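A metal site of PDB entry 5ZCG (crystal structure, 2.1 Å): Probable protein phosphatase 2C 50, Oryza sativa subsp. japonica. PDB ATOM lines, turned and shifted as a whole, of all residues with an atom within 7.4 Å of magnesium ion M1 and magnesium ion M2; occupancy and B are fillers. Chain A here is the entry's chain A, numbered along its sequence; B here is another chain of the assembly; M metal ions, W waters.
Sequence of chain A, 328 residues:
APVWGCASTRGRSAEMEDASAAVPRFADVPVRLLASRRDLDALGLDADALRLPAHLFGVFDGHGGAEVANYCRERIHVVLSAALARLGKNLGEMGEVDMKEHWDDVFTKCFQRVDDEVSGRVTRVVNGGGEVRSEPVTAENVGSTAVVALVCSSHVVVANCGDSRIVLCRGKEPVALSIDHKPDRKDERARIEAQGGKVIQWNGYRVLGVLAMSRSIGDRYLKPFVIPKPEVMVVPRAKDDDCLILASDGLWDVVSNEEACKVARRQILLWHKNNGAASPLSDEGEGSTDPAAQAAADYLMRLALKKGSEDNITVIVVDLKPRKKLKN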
ATOM      1  N   GLU A  15      -7.709 -18.285  15.194  1.00  0.00           N
ATOM      2  CA  GLU A  15      -8.260 -19.598  14.893  1.00  0.00           C
ATOM      3  C   GLU A  15      -7.469 -20.294  13.777  1.00  0.00           C
ATOM      4  O   GLU A  15      -6.789 -19.657  12.974  1.00  0.00           O
ATOM      5  CB  GLU A  15      -9.748 -19.498  14.510  1.00  0.00           C
ATOM      6  CG  GLU A  15     -10.643 -19.446  15.728  1.00  0.00           C
ATOM      7  CD  GLU A  15     -11.570 -18.244  15.743  1.00  0.00           C
ATOM      8  OE1 GLU A  15     -11.999 -17.836  16.836  1.00  0.00           O
ATOM      9  OE2 GLU A  15     -11.887 -17.718  14.646  1.00  0.00           O
ATOM     10  N   MET A  16      -7.591 -21.617  13.758  1.00  0.00           N
ATOM     11  CA  MET A  16      -6.907 -22.451  12.786  1.00  0.00           C
ATOM     12  C   MET A  16      -7.767 -22.634  11.543  1.00  0.00           C
ATOM     13  O   MET A  16      -8.901 -23.133  11.638  1.00  0.00           O
ATOM     14  CB  MET A  16      -6.568 -23.815  13.393  1.00  0.00           C
ATOM     15  CG  MET A  16      -5.911 -24.763  12.426  1.00  0.00           C
ATOM     16  SD  MET A  16      -4.399 -24.076  11.750  1.00  0.00           S
ATOM     17  CE  MET A  16      -3.379 -25.546  11.641  1.00  0.00           C
ATOM     18  N   GLU A  17      -7.239 -22.254  10.381  1.00  0.00           N
ATOM     19  CA  GLU A  17      -7.934 -22.438   9.117  1.00  0.00           C
ATOM     20  C   GLU A  17      -7.102 -23.190   8.087  1.00  0.00           C
ATOM     21  O   GLU A  17      -7.548 -23.345   6.942  1.00  0.00           O
ATOM     22  CB  GLU A  17      -8.351 -21.081   8.535  1.00  0.00           C
ATOM     23  CG  GLU A  17      -9.263 -20.298   9.484  1.00  0.00           C
ATOM     24  CD  GLU A  17      -9.597 -18.916   8.961  1.00  0.00           C
ATOM     25  OE1 GLU A  17     -10.604 -18.335   9.430  1.00  0.00           O
ATOM     26  OE2 GLU A  17      -8.874 -18.411   8.072  1.00  0.00           O
ATOM     27  N   ASP A  18      -5.911 -23.651   8.455  1.00  0.00           N
ATOM     28  CA  ASP A  18      -5.173 -24.602   7.645  1.00  0.00           C
ATOM     29  C   ASP A  18      -5.747 -26.000   7.863  1.00  0.00           C
ATOM     30  O   ASP A  18      -6.205 -26.335   8.970  1.00  0.00           O
ATOM     31  CB  ASP A  18      -3.689 -24.611   8.040  1.00  0.00           C
ATOM     32  CG  ASP A  18      -2.867 -23.568   7.313  1.00  0.00           C
ATOM     33  OD1 ASP A  18      -3.439 -22.647   6.694  1.00  0.00           O
ATOM     34  OD2 ASP A  18      -1.621 -23.658   7.397  1.00  0.00           O
ATOM     35  N   PHE A  60      -4.134 -27.473   2.509  1.00  0.00           N
ATOM     36  CA  PHE A  60      -5.259 -26.625   2.107  1.00  0.00           C
ATOM     37  C   PHE A  60      -5.303 -25.435   3.055  1.00  0.00           C
ATOM     38  O   PHE A  60      -5.657 -25.578   4.225  1.00  0.00           O
ATOM     39  CB  PHE A  60      -6.562 -27.418   2.142  1.00  0.00           C
ATOM     40  CG  PHE A  60      -6.429 -28.818   1.623  1.00  0.00           C
ATOM     41  CD1 PHE A  60      -6.425 -29.072   0.261  1.00  0.00           C
ATOM     42  CD2 PHE A  60      -6.249 -29.878   2.499  1.00  0.00           C
ATOM     43  CE1 PHE A  60      -6.283 -30.355  -0.222  1.00  0.00           C
ATOM     44  CE2 PHE A  60      -6.104 -31.172   2.023  1.00  0.00           C
ATOM     45  CZ  PHE A  60      -6.122 -31.403   0.654  1.00  0.00           C
ATOM     46  N   ASP A  61      -4.960 -24.264   2.549  1.00  0.00           N
ATOM     47  CA  ASP A  61      -4.877 -23.043   3.351  1.00  0.00           C
ATOM     48  C   ASP A  61      -6.193 -22.296   3.164  1.00  0.00           C
ATOM     49  O   ASP A  61      -6.429 -21.675   2.131  1.00  0.00           O
ATOM     50  CB  ASP A  61      -3.661 -22.226   2.914  1.00  0.00           C
ATOM     51  CG  ASP A  61      -3.489 -20.941   3.682  1.00  0.00           C
ATOM     52  OD1 ASP A  61      -4.385 -20.537   4.456  1.00  0.00           O
ATOM     53  OD2 ASP A  61      -2.419 -20.314   3.491  1.00  0.00           O
ATOM     54  N   GLY A  62      -7.063 -22.380   4.172  1.00  0.00           N
ATOM     55  CA  GLY A  62      -8.338 -21.708   4.097  1.00  0.00           C
ATOM     56  C   GLY A  62      -8.252 -20.235   4.482  1.00  0.00           C
ATOM     57  O   GLY A  62      -7.404 -19.820   5.255  1.00  0.00           O
ATOM     58  N   HIS A  63      -9.128 -19.442   3.861  1.00  0.00           N
ATOM     59  CA  HIS A  63      -9.339 -18.037   4.212  1.00  0.00           C
ATOM     60  C   HIS A  63     -10.838 -17.778   4.271  1.00  0.00           C
ATOM     61  O   HIS A  63     -11.639 -18.490   3.645  1.00  0.00           O
ATOM     62  CB  HIS A  63      -8.664 -17.077   3.216  1.00  0.00           C
ATOM     63  CG  HIS A  63      -9.020 -17.345   1.784  1.00  0.00           C
ATOM     64  ND1 HIS A  63      -8.226 -18.112   0.958  1.00  0.00           N
ATOM     65  CD2 HIS A  63     -10.089 -16.968   1.050  1.00  0.00           C
ATOM     66  CE1 HIS A  63      -8.792 -18.186  -0.236  1.00  0.00           C
ATOM     67  NE2 HIS A  63      -9.924 -17.498  -0.210  1.00  0.00           N
ATOM     68  N   GLY A  64     -11.228 -16.769   5.034  1.00  0.00           N
ATOM     69  CA  GLY A  64     -12.621 -16.503   5.324  1.00  0.00           C
ATOM     70  C   GLY A  64     -13.267 -17.473   6.290  1.00  0.00           C
ATOM     71  O   GLY A  64     -14.436 -17.301   6.646  1.00  0.00           O
ATOM     72  N   GLY A  65     -12.530 -18.466   6.741  1.00  0.00           N
ATOM     73  CA  GLY A  65     -13.068 -19.553   7.532  1.00  0.00           C
ATOM     74  C   GLY A  65     -12.289 -20.817   7.255  1.00  0.00           C
ATOM     75  O   GLY A  65     -11.419 -20.863   6.383  1.00  0.00           O
ATOM     76  N   ALA A  69     -11.303 -25.331   3.486  1.00  0.00           N
ATOM     77  CA  ALA A  69     -10.088 -26.119   3.679  1.00  0.00           C
ATOM     78  C   ALA A  69     -10.406 -27.516   4.235  1.00  0.00           C
ATOM     79  O   ALA A  69      -9.836 -28.517   3.785  1.00  0.00           O
ATOM     80  CB  ALA A  69      -9.124 -25.383   4.610  1.00  0.00           C
ATOM     81  N   GLY A 143     -12.803 -19.595   1.113  1.00  0.00           N
ATOM     82  CA  GLY A 143     -12.029 -20.308   0.119  1.00  0.00           C
ATOM     83  C   GLY A 143     -10.877 -21.072   0.732  1.00  0.00           C
ATOM     84  O   GLY A 143     -10.704 -21.117   1.952  1.00  0.00           O
ATOM     85  N   SER A 144     -10.066 -21.671  -0.145  1.00  0.00           N
ATOM     86  CA  SER A 144      -8.892 -22.384   0.318  1.00  0.00           C
ATOM     87  C   SER A 144      -7.926 -22.575  -0.840  1.00  0.00           C
ATOM     88  O   SER A 144      -8.342 -22.659  -2.006  1.00  0.00           O
ATOM     89  CB  SER A 144      -9.259 -23.729   0.927  1.00  0.00           C
ATOM     90  OG  SER A 144      -8.094 -24.477   1.223  1.00  0.00           O
ATOM     91  N   THR A 145      -6.636 -22.614  -0.519  1.00  0.00           N
ATOM     92  CA  THR A 145      -5.679 -23.143  -1.460  1.00  0.00           C
ATOM     93  C   THR A 145      -5.766 -24.665  -1.460  1.00  0.00           C
ATOM     94  O   THR A 145      -6.428 -25.279  -0.612  1.00  0.00           O
ATOM     95  CB  THR A 145      -4.253 -22.733  -1.103  1.00  0.00           C
ATOM     96  OG1 THR A 145      -3.764 -23.565  -0.042  1.00  0.00           O
ATOM     97  CG2 THR A 145      -4.225 -21.289  -0.653  1.00  0.00           C
ATOM     98  N   ASP A 163      -1.592 -20.119  -3.342  1.00  0.00           N
ATOM     99  CA  ASP A 163      -0.247 -19.704  -2.967  1.00  0.00           C
ATOM    100  C   ASP A 163       0.382 -20.584  -1.896  1.00  0.00           C
ATOM    101  O   ASP A 163       1.381 -20.188  -1.295  1.00  0.00           O
ATOM    102  CB  ASP A 163      -0.242 -18.236  -2.524  1.00  0.00           C
ATOM    103  CG  ASP A 163      -1.135 -17.961  -1.329  1.00  0.00           C
ATOM    104  OD1 ASP A 163      -1.563 -18.916  -0.650  1.00  0.00           O
ATOM    105  OD2 ASP A 163      -1.429 -16.772  -1.088  1.00  0.00           O
ATOM    106  N   SER A 164      -0.182 -21.759  -1.634  1.00  0.00           N
ATOM    107  CA  SER A 164       0.603 -22.766  -0.960  1.00  0.00           C
ATOM    108  C   SER A 164       1.605 -23.335  -1.962  1.00  0.00           C
ATOM    109  O   SER A 164       1.528 -23.090  -3.171  1.00  0.00           O
ATOM    110  CB  SER A 164      -0.302 -23.868  -0.394  1.00  0.00           C
ATOM    111  OG  SER A 164      -1.192 -23.353   0.577  1.00  0.00           O
ATOM    112  N   SER A 248       1.675 -24.546   3.667  1.00  0.00           N
ATOM    113  CA  SER A 248       0.971 -23.298   3.429  1.00  0.00           C
ATOM    114  C   SER A 248       1.959 -22.135   3.492  1.00  0.00           C
ATOM    115  O   SER A 248       3.112 -22.283   3.906  1.00  0.00           O
ATOM    116  CB  SER A 248      -0.134 -23.115   4.468  1.00  0.00           C
ATOM    117  OG  SER A 248       0.385 -23.137   5.780  1.00  0.00           O
ATOM    118  N   ASP A 249       1.488 -20.960   3.069  1.00  0.00           N
ATOM    119  CA  ASP A 249       2.359 -19.793   3.065  1.00  0.00           C
ATOM    120  C   ASP A 249       2.821 -19.401   4.457  1.00  0.00           C
ATOM    121  O   ASP A 249       3.736 -18.574   4.572  1.00  0.00           O
ATOM    122  CB  ASP A 249       1.666 -18.603   2.371  1.00  0.00           C
ATOM    123  CG  ASP A 249       0.354 -18.215   3.042  1.00  0.00           C
ATOM    124  OD1 ASP A 249      -0.072 -18.890   4.003  1.00  0.00           O
ATOM    125  OD2 ASP A 249      -0.269 -17.234   2.589  1.00  0.00           O
ATOM    126  N   GLY A 250       2.222 -19.956   5.516  1.00  0.00           N
ATOM    127  CA  GLY A 250       2.755 -19.747   6.853  1.00  0.00           C
ATOM    128  C   GLY A 250       4.216 -20.149   6.983  1.00  0.00           C
ATOM    129  O   GLY A 250       4.933 -19.603   7.822  1.00  0.00           O
ATOM    130  N   LEU A 251       4.661 -21.112   6.173  1.00  0.00           N
ATOM    131  CA  LEU A 251       6.072 -21.446   6.100  1.00  0.00           C
ATOM    132  C   LEU A 251       6.799 -20.569   5.083  1.00  0.00           C
ATOM    133  O   LEU A 251       7.759 -19.867   5.421  1.00  0.00           O
ATOM    134  CB  LEU A 251       6.254 -22.929   5.746  1.00  0.00           C
ATOM    135  CG  LEU A 251       7.711 -23.391   5.579  1.00  0.00           C
ATOM    136  CD1 LEU A 251       8.496 -23.120   6.862  1.00  0.00           C
ATOM    137  CD2 LEU A 251       7.800 -24.867   5.207  1.00  0.00           C
ATOM    138  N   ASP A 253       6.258 -17.797   3.597  1.00  0.00           N
ATOM    139  CA  ASP A 253       6.381 -16.351   3.751  1.00  0.00           C
ATOM    140  C   ASP A 253       7.682 -15.958   4.436  1.00  0.00           C
ATOM    141  O   ASP A 253       8.231 -14.895   4.150  1.00  0.00           O
ATOM    142  CB  ASP A 253       5.174 -15.801   4.516  1.00  0.00           C
ATOM    143  CG  ASP A 253       3.933 -15.651   3.638  1.00  0.00           C
ATOM    144  OD1 ASP A 253       4.088 -15.578   2.400  1.00  0.00           O
ATOM    145  OD2 ASP A 253       2.808 -15.597   4.186  1.00  0.00           O
ATOM    146  N   ASP A 311       0.963 -16.302  10.491  1.00  0.00           N
ATOM    147  CA  ASP A 311      -0.153 -17.084   9.991  1.00  0.00           C
ATOM    148  C   ASP A 311      -0.225 -18.480  10.620  1.00  0.00           C
ATOM    149  O   ASP A 311       0.665 -18.909  11.362  1.00  0.00           O
ATOM    150  CB  ASP A 311      -0.038 -17.218   8.469  1.00  0.00           C
ATOM    151  CG  ASP A 311      -1.373 -17.419   7.797  1.00  0.00           C
ATOM    152  OD1 ASP A 311      -2.367 -17.728   8.485  1.00  0.00           O
ATOM    153  OD2 ASP A 311      -1.407 -17.285   6.564  1.00  0.00           O
ATOM    154  N   ASN A 312      -1.312 -19.181  10.299  1.00  0.00           N
ATOM    155  CA  ASN A 312      -1.326 -20.621  10.486  1.00  0.00           C
ATOM    156  C   ASN A 312      -0.152 -21.213   9.709  1.00  0.00           C
ATOM    157  O   ASN A 312       0.238 -20.716   8.650  1.00  0.00           O
ATOM    158  CB  ASN A 312      -2.634 -21.233   9.979  1.00  0.00           C
ATOM    159  CG  ASN A 312      -3.871 -20.587  10.578  1.00  0.00           C
ATOM    160  OD1 ASN A 312      -4.955 -20.639   9.982  1.00  0.00           O
ATOM    161  ND2 ASN A 312      -3.735 -19.992  11.750  1.00  0.00           N
ATOM    162  N   ILE A 313       0.419 -22.286  10.258  1.00  0.00           N
ATOM    163  CA  ILE A 313       1.547 -22.958   9.637  1.00  0.00           C
ATOM    164  C   ILE A 313       1.216 -24.437   9.536  1.00  0.00           C
ATOM    165  O   ILE A 313       0.867 -25.065  10.543  1.00  0.00           O
ATOM    166  CB  ILE A 313       2.856 -22.754  10.425  1.00  0.00           C
ATOM    167  CG1 ILE A 313       3.150 -21.263  10.632  1.00  0.00           C
ATOM    168  CG2 ILE A 313       4.015 -23.428   9.701  1.00  0.00           C
ATOM    169  CD1 ILE A 313       4.100 -20.979  11.790  1.00  0.00           C
ATOM    170  N   SER B  71     -10.208 -13.672   7.621  1.00  0.00           N
ATOM    171  CA  SER B  71      -8.899 -13.775   7.005  1.00  0.00           C
ATOM    172  C   SER B  71      -8.984 -13.660   5.482  1.00  0.00           C
ATOM    173  O   SER B  71     -10.063 -13.745   4.885  1.00  0.00           O
ATOM    174  CB  SER B  71      -8.246 -15.104   7.386  1.00  0.00           C
ATOM    175  OG  SER B  71      -9.159 -16.177   7.199  1.00  0.00           O
ATOM    176  N   GLY B  72      -7.819 -13.477   4.857  1.00  0.00           N
ATOM    177  CA  GLY B  72      -7.723 -13.319   3.422  1.00  0.00           C
ATOM    178  C   GLY B  72      -7.814 -11.887   2.914  1.00  0.00           C
ATOM    179  O   GLY B  72      -7.527 -11.651   1.733  1.00  0.00           O
HETATM  180 MG    MG M   1      -1.794 -18.861   5.138  1.00  0.00          MG
HETATM  181 MG    MG M   2      -5.461 -19.103   5.805  1.00  0.00          MG
HETATM  182  O   HOH W   1      -5.045 -17.306   4.529  1.00  0.00           O
HETATM  183  O   HOH W   2      -6.415 -17.954   7.540  1.00  0.00           O
HETATM  184  O   HOH W   3      -4.977 -20.723   6.880  1.00  0.00           O
HETATM  185  O   HOH W   4      -1.231 -20.552   6.256  1.00  0.00           O
HETATM  186  O   HOH W   5      -2.344 -17.300   4.180  1.00  0.00           O
HETATM  187  O   HOH W   6      -3.525 -18.398   6.153  1.00  0.00           O
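Water W4 lies within hydrogen-bond range of O of Asn 312 (2.8 Å), OD1 of Asp 18 (3.1 Å) and OG of Ser 248 (3.1 Å). Water W2 bridges OE2 of Glu 17 (2.6 Å) and OG of Ser 71 of chain B (3.3 Å). Water W3 bridges OD1 of Asp 18 (2.5 Å) and OD1 of Asn 312 (3.1 Å).
Magnesium ion M1 is bound by water W5 (1.9 Å), water W6 (2.1 Å), OD1 of Asp 249 (2.1 Å), water W4 (2.1 Å), OD2 of Asp 311 (2.2 Å) and OD2 of Asp 61 (2.3 Å). Magnesium ion M1 has six donor atoms within binding distance.
Magnesium ion M2 is bound by water W3 (2.0 Å), water W6 (2.1 Å), the backbone carbonyl oxygen (O) of Gly 62 (2.1 Å), water W1 (2.2 Å), the side-chain carboxylate (OD1) of Asp 61 (2.2 Å) and water W2 (2.3 Å).
Within 4 Å of magnesium ion M1: Asp 61, Asp 249 and Asp 311.
O of Asp 61 sits at hydrogen-bond distance from N of Thr 145, at 2.8 Å. N of Gly 62 lies within hydrogen-bond range of O of Glu 17 (3.0 Å). The backbone carbonyl oxygen (O) of Asp 61 sits close to the side-chain hydroxyl (OG) of Ser 144 (3.4 Å).
Within 4 Å of magnesium ion M2: Asp 61 and Gly 62. The nearest printed residue that does not touch magnesium ion M2 is Glu 17 (4.2 Å).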
